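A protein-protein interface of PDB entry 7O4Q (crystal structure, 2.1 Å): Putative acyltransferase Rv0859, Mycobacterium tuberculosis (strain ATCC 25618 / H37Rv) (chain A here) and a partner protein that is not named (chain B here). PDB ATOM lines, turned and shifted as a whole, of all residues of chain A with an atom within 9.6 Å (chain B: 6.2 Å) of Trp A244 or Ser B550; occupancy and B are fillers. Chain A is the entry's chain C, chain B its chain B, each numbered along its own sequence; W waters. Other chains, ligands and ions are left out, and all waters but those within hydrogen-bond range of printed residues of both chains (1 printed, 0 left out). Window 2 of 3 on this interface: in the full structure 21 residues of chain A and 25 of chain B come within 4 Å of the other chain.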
ATOM      1  N   LEU A 155     -23.473   7.506  -7.851  1.00  0.00           N
ATOM      2  CA  LEU A 155     -22.072   7.378  -7.462  1.00  0.00           C
ATOM      3  C   LEU A 155     -21.900   7.570  -5.960  1.00  0.00           C
ATOM      4  O   LEU A 155     -21.101   6.870  -5.330  1.00  0.00           O
ATOM      5  CB  LEU A 155     -21.217   8.378  -8.241  1.00  0.00           C
ATOM      6  CG  LEU A 155     -19.705   8.343  -8.006  1.00  0.00           C
ATOM      7  CD1 LEU A 155     -19.126   6.965  -8.306  1.00  0.00           C
ATOM      8  CD2 LEU A 155     -19.021   9.410  -8.848  1.00  0.00           C
ATOM      9  N   ILE A 156     -22.645   8.506  -5.369  1.00  0.00           N
ATOM     10  CA  ILE A 156     -22.601   8.690  -3.921  1.00  0.00           C
ATOM     11  C   ILE A 156     -23.011   7.405  -3.212  1.00  0.00           C
ATOM     12  O   ILE A 156     -22.333   6.937  -2.290  1.00  0.00           O
ATOM     13  CB  ILE A 156     -23.495   9.869  -3.501  1.00  0.00           C
ATOM     14  CG1 ILE A 156     -22.902  11.198  -3.974  1.00  0.00           C
ATOM     15  CG2 ILE A 156     -23.698   9.870  -1.993  1.00  0.00           C
ATOM     16  CD1 ILE A 156     -23.835  12.383  -3.779  1.00  0.00           C
ATOM     17  N   THR A 158     -22.835   4.455  -4.338  1.00  0.00           N
ATOM     18  CA  THR A 158     -21.813   3.437  -4.559  1.00  0.00           C
ATOM     19  C   THR A 158     -20.615   3.648  -3.644  1.00  0.00           C
ATOM     20  O   THR A 158     -20.084   2.688  -3.074  1.00  0.00           O
ATOM     21  CB  THR A 158     -21.367   3.442  -6.022  1.00  0.00           C
ATOM     22  OG1 THR A 158     -22.510   3.327  -6.878  1.00  0.00           O
ATOM     23  CG2 THR A 158     -20.427   2.279  -6.290  1.00  0.00           C
ATOM     24  N   ILE A 159     -20.172   4.899  -3.494  1.00  0.00           N
ATOM     25  CA  ILE A 159     -18.992   5.176  -2.682  1.00  0.00           C
ATOM     26  C   ILE A 159     -19.289   4.949  -1.206  1.00  0.00           C
ATOM     27  O   ILE A 159     -18.455   4.414  -0.467  1.00  0.00           O
ATOM     28  CB  ILE A 159     -18.491   6.607  -2.946  1.00  0.00           C
ATOM     29  CG1 ILE A 159     -18.064   6.764  -4.406  1.00  0.00           C
ATOM     30  CG2 ILE A 159     -17.332   6.947  -2.021  1.00  0.00           C
ATOM     31  CD1 ILE A 159     -17.803   8.199  -4.810  1.00  0.00           C
ATOM     32  N   GLU A 160     -20.477   5.347  -0.750  1.00  0.00           N
ATOM     33  CA  GLU A 160     -20.823   5.257   0.663  1.00  0.00           C
ATOM     34  C   GLU A 160     -21.443   3.922   1.050  1.00  0.00           C
ATOM     35  O   GLU A 160     -21.672   3.688   2.241  1.00  0.00           O
ATOM     36  CB  GLU A 160     -21.782   6.391   1.046  1.00  0.00           C
ATOM     37  CG  GLU A 160     -21.290   7.785   0.676  1.00  0.00           C
ATOM     38  CD  GLU A 160     -20.040   8.199   1.434  1.00  0.00           C
ATOM     39  OE1 GLU A 160     -19.751   7.606   2.496  1.00  0.00           O
ATOM     40  OE2 GLU A 160     -19.345   9.124   0.965  1.00  0.00           O
ATOM     41  N   ALA A 238     -17.900   9.891 -15.192  1.00  0.00           N
ATOM     42  CA  ALA A 238     -17.856   9.978 -13.734  1.00  0.00           C
ATOM     43  C   ALA A 238     -16.735   9.121 -13.159  1.00  0.00           C
ATOM     44  O   ALA A 238     -16.040   9.539 -12.226  1.00  0.00           O
ATOM     45  CB  ALA A 238     -19.202   9.562 -13.139  1.00  0.00           C
ATOM     46  N   LEU A 239     -16.540   7.920 -13.702  1.00  0.00           N
ATOM     47  CA  LEU A 239     -15.506   7.035 -13.181  1.00  0.00           C
ATOM     48  C   LEU A 239     -14.104   7.447 -13.614  1.00  0.00           C
ATOM     49  O   LEU A 239     -13.128   6.975 -13.024  1.00  0.00           O
ATOM     50  CB  LEU A 239     -15.787   5.593 -13.605  1.00  0.00           C
ATOM     51  CG  LEU A 239     -17.107   5.026 -13.072  1.00  0.00           C
ATOM     52  CD1 LEU A 239     -17.269   3.557 -13.441  1.00  0.00           C
ATOM     53  CD2 LEU A 239     -17.209   5.220 -11.564  1.00  0.00           C
ATOM     54  N   GLN A 240     -13.975   8.311 -14.625  1.00  0.00           N
ATOM     55  CA  GLN A 240     -12.649   8.803 -14.988  1.00  0.00           C
ATOM     56  C   GLN A 240     -12.105   9.743 -13.920  1.00  0.00           C
ATOM     57  O   GLN A 240     -10.896   9.761 -13.658  1.00  0.00           O
ATOM     58  CB  GLN A 240     -12.689   9.494 -16.354  1.00  0.00           C
ATOM     59  CG  GLN A 240     -12.763   8.518 -17.521  1.00  0.00           C
ATOM     60  CD  GLN A 240     -12.995   9.201 -18.859  1.00  0.00           C
ATOM     61  OE1 GLN A 240     -12.906  10.424 -18.972  1.00  0.00           O
ATOM     62  NE2 GLN A 240     -13.301   8.408 -19.882  1.00  0.00           N
ATOM     63  N   LYS A 241     -12.982  10.526 -13.288  1.00  0.00           N
ATOM     64  CA  LYS A 241     -12.563  11.330 -12.145  1.00  0.00           C
ATOM     65  C   LYS A 241     -12.486  10.487 -10.876  1.00  0.00           C
ATOM     66  O   LYS A 241     -11.489  10.537 -10.150  1.00  0.00           O
ATOM     67  CB  LYS A 241     -13.513  12.512 -11.945  1.00  0.00           C
ATOM     68  CG  LYS A 241     -13.371  13.152 -10.573  1.00  0.00           C
ATOM     69  CD  LYS A 241     -13.976  14.542 -10.512  1.00  0.00           C
ATOM     70  CE  LYS A 241     -13.047  15.582 -11.120  1.00  0.00           C
ATOM     71  NZ  LYS A 241     -11.738  15.662 -10.412  1.00  0.00           N
ATOM     72  N   TYR A 242     -13.527   9.701 -10.597  1.00  0.00           N
ATOM     73  CA  TYR A 242     -13.538   8.821  -9.426  1.00  0.00           C
ATOM     74  C   TYR A 242     -12.974   7.453  -9.816  1.00  0.00           C
ATOM     75  O   TYR A 242     -13.658   6.428  -9.834  1.00  0.00           O
ATOM     76  CB  TYR A 242     -14.945   8.728  -8.848  1.00  0.00           C
ATOM     77  CG  TYR A 242     -15.369  10.016  -8.180  1.00  0.00           C
ATOM     78  CD1 TYR A 242     -15.893  11.069  -8.921  1.00  0.00           C
ATOM     79  CD2 TYR A 242     -15.214  10.191  -6.811  1.00  0.00           C
ATOM     80  CE1 TYR A 242     -16.265  12.251  -8.314  1.00  0.00           C
ATOM     81  CE2 TYR A 242     -15.584  11.369  -6.196  1.00  0.00           C
ATOM     82  CZ  TYR A 242     -16.107  12.395  -6.952  1.00  0.00           C
ATOM     83  OH  TYR A 242     -16.473  13.570  -6.336  1.00  0.00           O
ATOM     84  N   HIS A 243     -11.672   7.462 -10.111  1.00  0.00           N
ATOM     85  CA  HIS A 243     -11.009   6.338 -10.761  1.00  0.00           C
ATOM     86  C   HIS A 243     -10.838   5.121  -9.863  1.00  0.00           C
ATOM     87  O   HIS A 243     -10.512   4.046 -10.376  1.00  0.00           O
ATOM     88  CB  HIS A 243      -9.646   6.783 -11.295  1.00  0.00           C
ATOM     89  CG  HIS A 243      -8.798   7.490 -10.283  1.00  0.00           C
ATOM     90  ND1 HIS A 243      -8.154   6.829  -9.259  1.00  0.00           N
ATOM     91  CD2 HIS A 243      -8.483   8.799 -10.142  1.00  0.00           C
ATOM     92  CE1 HIS A 243      -7.481   7.701  -8.531  1.00  0.00           C
ATOM     93  NE2 HIS A 243      -7.666   8.904  -9.044  1.00  0.00           N
ATOM     94  N   TRP A 244     -11.042   5.250  -8.555  1.00  0.00           N
ATOM     95  CA  TRP A 244     -10.965   4.106  -7.656  1.00  0.00           C
ATOM     96  C   TRP A 244     -12.280   3.344  -7.558  1.00  0.00           C
ATOM     97  O   TRP A 244     -12.332   2.307  -6.888  1.00  0.00           O
ATOM     98  CB  TRP A 244     -10.523   4.554  -6.259  1.00  0.00           C
ATOM     99  CG  TRP A 244     -11.400   5.618  -5.672  1.00  0.00           C
ATOM    100  CD1 TRP A 244     -12.468   5.436  -4.844  1.00  0.00           C
ATOM    101  CD2 TRP A 244     -11.282   7.032  -5.873  1.00  0.00           C
ATOM    102  NE1 TRP A 244     -13.021   6.650  -4.515  1.00  0.00           N
ATOM    103  CE2 TRP A 244     -12.311   7.645  -5.134  1.00  0.00           C
ATOM    104  CE3 TRP A 244     -10.402   7.838  -6.604  1.00  0.00           C
ATOM    105  CZ2 TRP A 244     -12.489   9.027  -5.105  1.00  0.00           C
ATOM    106  CZ3 TRP A 244     -10.581   9.210  -6.575  1.00  0.00           C
ATOM    107  CH2 TRP A 244     -11.616   9.790  -5.830  1.00  0.00           C
ATOM    108  N   VAL A 245     -13.337   3.828  -8.203  1.00  0.00           N
ATOM    109  CA  VAL A 245     -14.628   3.152  -8.232  1.00  0.00           C
ATOM    110  C   VAL A 245     -14.726   2.381  -9.541  1.00  0.00           C
ATOM    111  O   VAL A 245     -14.606   2.964 -10.625  1.00  0.00           O
ATOM    112  CB  VAL A 245     -15.790   4.148  -8.087  1.00  0.00           C
ATOM    113  CG1 VAL A 245     -17.118   3.418  -8.159  1.00  0.00           C
ATOM    114  CG2 VAL A 245     -15.667   4.917  -6.781  1.00  0.00           C
ATOM    115  N   GLU A 246     -14.946   1.071  -9.442  1.00  0.00           N
ATOM    116  CA  GLU A 246     -14.983   0.221 -10.627  1.00  0.00           C
ATOM    117  C   GLU A 246     -16.296   0.369 -11.388  1.00  0.00           C
ATOM    118  O   GLU A 246     -16.295   0.516 -12.616  1.00  0.00           O
ATOM    119  CB  GLU A 246     -14.766  -1.239 -10.228  1.00  0.00           C
ATOM    120  CG  GLU A 246     -14.815  -2.206 -11.396  1.00  0.00           C
ATOM    121  CD  GLU A 246     -14.787  -3.655 -10.956  1.00  0.00           C
ATOM    122  OE1 GLU A 246     -15.107  -3.928  -9.779  1.00  0.00           O
ATOM    123  OE2 GLU A 246     -14.444  -4.521 -11.787  1.00  0.00           O
ATOM    124  N   LYS A 247     -17.423   0.326 -10.678  1.00  0.00           N
ATOM    125  CA  LYS A 247     -18.736   0.295 -11.306  1.00  0.00           C
ATOM    126  C   LYS A 247     -19.733   1.068 -10.453  1.00  0.00           C
ATOM    127  O   LYS A 247     -19.713   0.975  -9.223  1.00  0.00           O
ATOM    128  CB  LYS A 247     -19.212  -1.152 -11.502  1.00  0.00           C
ATOM    129  CG  LYS A 247     -20.632  -1.292 -12.034  1.00  0.00           C
ATOM    130  CD  LYS A 247     -21.050  -2.756 -12.097  1.00  0.00           C
ATOM    131  CE  LYS A 247     -22.499  -2.906 -12.540  1.00  0.00           C
ATOM    132  NZ  LYS A 247     -22.925  -4.335 -12.570  1.00  0.00           N
ATOM    133  N   ILE A 248     -20.610   1.819 -11.114  1.00  0.00           N
ATOM    134  CA  ILE A 248     -21.630   2.605 -10.431  1.00  0.00           C
ATOM    135  C   ILE A 248     -22.866   1.742 -10.224  1.00  0.00           C
ATOM    136  O   ILE A 248     -23.369   1.119 -11.166  1.00  0.00           O
ATOM    137  CB  ILE A 248     -21.971   3.876 -11.227  1.00  0.00           C
ATOM    138  CG1 ILE A 248     -20.827   4.884 -11.127  1.00  0.00           C
ATOM    139  CG2 ILE A 248     -23.273   4.491 -10.730  1.00  0.00           C
ATOM    140  CD1 ILE A 248     -21.125   6.211 -11.788  1.00  0.00           C
ATOM    141  N   ASP A 295     -16.951  19.015  -5.479  1.00  0.00           N
ATOM    142  CA  ASP A 295     -16.662  18.590  -6.843  1.00  0.00           C
ATOM    143  C   ASP A 295     -17.912  18.668  -7.721  1.00  0.00           C
ATOM    144  O   ASP A 295     -18.975  18.162  -7.328  1.00  0.00           O
ATOM    145  CB  ASP A 295     -16.112  17.166  -6.840  1.00  0.00           C
ATOM    146  CG  ASP A 295     -16.138  16.528  -8.211  1.00  0.00           C
ATOM    147  OD1 ASP A 295     -15.488  17.068  -9.131  1.00  0.00           O
ATOM    148  OD2 ASP A 295     -16.809  15.486  -8.368  1.00  0.00           O
ATOM    149  N   ILE A 298     -19.431  14.840  -9.137  1.00  0.00           N
ATOM    150  CA  ILE A 298     -20.380  14.193  -8.237  1.00  0.00           C
ATOM    151  C   ILE A 298     -21.528  15.144  -7.910  1.00  0.00           C
ATOM    152  O   ILE A 298     -22.633  14.702  -7.569  1.00  0.00           O
ATOM    153  CB  ILE A 298     -19.658  13.692  -6.970  1.00  0.00           C
ATOM    154  CG1 ILE A 298     -20.439  12.550  -6.320  1.00  0.00           C
ATOM    155  CG2 ILE A 298     -19.443  14.827  -5.973  1.00  0.00           C
ATOM    156  CD1 ILE A 298     -19.668  11.850  -5.222  1.00  0.00           C
ATOM    157  N   VAL B 546      -2.178  -0.041  -4.335  1.00  0.00           N
ATOM    158  CA  VAL B 546      -2.992   0.877  -5.126  1.00  0.00           C
ATOM    159  C   VAL B 546      -4.261   0.162  -5.569  1.00  0.00           C
ATOM    160  O   VAL B 546      -4.237  -1.031  -5.901  1.00  0.00           O
ATOM    161  CB  VAL B 546      -2.192   1.408  -6.331  1.00  0.00           C
ATOM    162  CG1 VAL B 546      -3.012   2.423  -7.116  1.00  0.00           C
ATOM    163  CG2 VAL B 546      -0.872   2.023  -5.872  1.00  0.00           C
ATOM    164  N   GLU B 547      -5.376   0.889  -5.569  1.00  0.00           N
ATOM    165  CA  GLU B 547      -6.661   0.312  -5.945  1.00  0.00           C
ATOM    166  C   GLU B 547      -6.591  -0.278  -7.350  1.00  0.00           C
ATOM    167  O   GLU B 547      -6.083   0.380  -8.268  1.00  0.00           O
ATOM    168  CB  GLU B 547      -7.766   1.368  -5.887  1.00  0.00           C
ATOM    169  CG  GLU B 547      -8.201   1.759  -4.484  1.00  0.00           C
ATOM    170  CD  GLU B 547      -9.041   0.689  -3.806  1.00  0.00           C
ATOM    171  OE1 GLU B 547      -9.413  -0.303  -4.470  1.00  0.00           O
ATOM    172  OE2 GLU B 547      -9.332   0.846  -2.602  1.00  0.00           O
ATOM    173  N   PRO B 548      -7.088  -1.502  -7.560  1.00  0.00           N
ATOM    174  CA  PRO B 548      -7.082  -2.069  -8.921  1.00  0.00           C
ATOM    175  C   PRO B 548      -7.826  -1.215  -9.929  1.00  0.00           C
ATOM    176  O   PRO B 548      -7.416  -1.142 -11.095  1.00  0.00           O
ATOM    177  CB  PRO B 548      -7.755  -3.435  -8.733  1.00  0.00           C
ATOM    178  CG  PRO B 548      -7.568  -3.760  -7.288  1.00  0.00           C
ATOM    179  CD  PRO B 548      -7.608  -2.452  -6.562  1.00  0.00           C
ATOM    180  N   ALA B 549      -8.916  -0.566  -9.511  1.00  0.00           N
ATOM    181  CA  ALA B 549      -9.680   0.269 -10.431  1.00  0.00           C
ATOM    182  C   ALA B 549      -8.872   1.481 -10.877  1.00  0.00           C
ATOM    183  O   ALA B 549      -8.923   1.866 -12.050  1.00  0.00           O
ATOM    184  CB  ALA B 549     -10.995   0.702  -9.778  1.00  0.00           C
ATOM    185  N   SER B 550      -8.122   2.096  -9.958  1.00  0.00           N
ATOM    186  CA  SER B 550      -7.273   3.223 -10.333  1.00  0.00           C
ATOM    187  C   SER B 550      -6.190   2.793 -11.313  1.00  0.00           C
ATOM    188  O   SER B 550      -5.837   3.546 -12.230  1.00  0.00           O
ATOM    189  CB  SER B 550      -6.644   3.848  -9.087  1.00  0.00           C
ATOM    190  OG  SER B 550      -7.629   4.381  -8.221  1.00  0.00           O
ATOM    191  N   ILE B 551      -5.651   1.585 -11.132  1.00  0.00           N
ATOM    192  CA  ILE B 551      -4.615   1.077 -12.029  1.00  0.00           C
ATOM    193  C   ILE B 551      -5.155   0.927 -13.445  1.00  0.00           C
ATOM    194  O   ILE B 551      -4.482   1.276 -14.423  1.00  0.00           O
ATOM    195  CB  ILE B 551      -4.056  -0.253 -11.488  1.00  0.00           C
ATOM    196  CG1 ILE B 551      -3.352  -0.026 -10.149  1.00  0.00           C
ATOM    197  CG2 ILE B 551      -3.110  -0.887 -12.497  1.00  0.00           C
ATOM    198  CD1 ILE B 551      -2.926  -1.299  -9.457  1.00  0.00           C
ATOM    199  N   GLU B 552      -6.379   0.407 -13.578  1.00  0.00           N
ATOM    200  CA  GLU B 552      -6.979   0.261 -14.900  1.00  0.00           C
ATOM    201  C   GLU B 552      -7.303   1.618 -15.514  1.00  0.00           C
ATOM    202  O   GLU B 552      -7.100   1.824 -16.716  1.00  0.00           O
ATOM    203  CB  GLU B 552      -8.235  -0.607 -14.815  1.00  0.00           C
ATOM    204  CG  GLU B 552      -7.994  -2.023 -14.288  1.00  0.00           C
ATOM    205  CD  GLU B 552      -7.124  -2.865 -15.211  1.00  0.00           C
ATOM    206  OE1 GLU B 552      -5.908  -2.596 -15.317  1.00  0.00           O
ATOM    207  OE2 GLU B 552      -7.658  -3.806 -15.837  1.00  0.00           O
ATOM    208  N   GLN B 553      -7.814   2.552 -14.706  1.00  0.00           N
ATOM    209  CA  GLN B 553      -8.090   3.897 -15.204  1.00  0.00           C
ATOM    210  C   GLN B 553      -6.810   4.598 -15.648  1.00  0.00           C
ATOM    211  O   GLN B 553      -6.796   5.284 -16.676  1.00  0.00           O
ATOM    212  CB  GLN B 553      -8.803   4.719 -14.131  1.00  0.00           C
ATOM    213  CG  GLN B 553     -10.285   4.418 -13.990  1.00  0.00           C
ATOM    214  CD  GLN B 553     -11.119   5.047 -15.092  1.00  0.00           C
ATOM    215  OE1 GLN B 553     -10.611   5.812 -15.914  1.00  0.00           O
ATOM    216  NE2 GLN B 553     -12.410   4.729 -15.111  1.00  0.00           N
ATOM    217  N   ALA B 554      -5.727   4.443 -14.884  1.00  0.00           N
ATOM    218  CA  ALA B 554      -4.460   5.050 -15.277  1.00  0.00           C
ATOM    219  C   ALA B 554      -4.005   4.535 -16.638  1.00  0.00           C
ATOM    220  O   ALA B 554      -3.483   5.300 -17.458  1.00  0.00           O
ATOM    221  CB  ALA B 554      -3.395   4.784 -14.213  1.00  0.00           C
ATOM    222  N   GLY B 555      -4.208   3.243 -16.903  1.00  0.00           N
ATOM    223  CA  GLY B 555      -3.844   2.699 -18.202  1.00  0.00           C
ATOM    224  C   GLY B 555      -4.680   3.272 -19.333  1.00  0.00           C
ATOM    225  O   GLY B 555      -4.148   3.678 -20.370  1.00  0.00           O
ATOM    226  N   LEU B 648      -3.065  10.127  -9.753  1.00  0.00           N
ATOM    227  CA  LEU B 648      -3.307   9.391 -10.989  1.00  0.00           C
ATOM    228  C   LEU B 648      -2.244   9.704 -12.033  1.00  0.00           C
ATOM    229  O   LEU B 648      -1.818   8.816 -12.781  1.00  0.00           O
ATOM    230  CB  LEU B 648      -4.701   9.710 -11.533  1.00  0.00           C
ATOM    231  CG  LEU B 648      -5.155   8.860 -12.724  1.00  0.00           C
ATOM    232  CD1 LEU B 648      -5.345   7.409 -12.306  1.00  0.00           C
ATOM    233  CD2 LEU B 648      -6.432   9.415 -13.341  1.00  0.00           C
ATOM    234  N   MET B 651       0.719   7.584 -11.504  1.00  0.00           N
ATOM    235  CA  MET B 651       0.474   6.234 -12.003  1.00  0.00           C
ATOM    236  C   MET B 651       0.578   6.186 -13.520  1.00  0.00           C
ATOM    237  O   MET B 651       1.162   5.250 -14.082  1.00  0.00           O
ATOM    238  CB  MET B 651      -0.900   5.754 -11.542  1.00  0.00           C
ATOM    239  CG  MET B 651      -1.117   5.849 -10.040  1.00  0.00           C
ATOM    240  SD  MET B 651      -2.788   5.370  -9.555  1.00  0.00           S
ATOM    241  CE  MET B 651      -2.959   3.841 -10.461  1.00  0.00           C
HETATM  242  O   HOH W   1     -12.871   3.292 -12.417  1.00  0.00           O
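Among the printed residues, merely in contact across the chains: Trp A244 with Ser B550 (3.4 Å), Trp A244 with Ala B549 (3.6 Å), His A243 with Gln B553 (3.6 Å), Gln A240 with Gln B553 (3.7 Å), His A243 with Leu B648 (3.8 Å) and Glu A246 with Ala B549 (3.98 Å).
Water W1 lies within hydrogen-bond range of O of Val A245 (2.5 Å), NE2 of Gln B553 (3.1 Å) and O of His A243 (3.2 Å).
Printed residues of chain A that touch a printed residue of chain B: Leu A239, Gln A240, His A243, Trp A244 and Glu A246.
Hydrophobic or aromatic side chains of chain A that line the printed part of chain B: Leu A239, His A243 and Trp A244.
Of the 12 printed residues of chain B, 4 touch a printed residue of chain A.
Of chain B, only Ala B549 (3.6 Å) and Ser B550 (3.4 Å) come within 4 Å of Trp A244.
Of chain A, only His A243 and Trp A244 come within 4 Å of Ser B550.
Of the printed residues of chain B, Gln A240 touches Gln B553 (3.7 Å).
Printed residues of chain A within 4 Å of Ala B549: His A243, Trp A244 and Glu A246.
The nearest residue of chain B that does not touch Trp A244 is Glu B547 (4.04 Å).
The nearest residue of chain A that does not touch Ser B550 is Val A245 (5.7 Å).
The nearest printed residue of chain B that does not touch His A243 is Met B651 (5.3 Å).
The side-chain hydroxyl (OG) of Ser B550 lies within hydrogen-bond range of a ring nitrogen (ND1) of His A243 (2.7 Å).
The backbone carbonyl oxygen of His A243 lies close to the backbone carbonyl oxygen of Ala B549 (3.2 Å).
O of Leu A239 sits at hydrogen-bond distance from NE2 of Gln B553 (3.1 Å).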
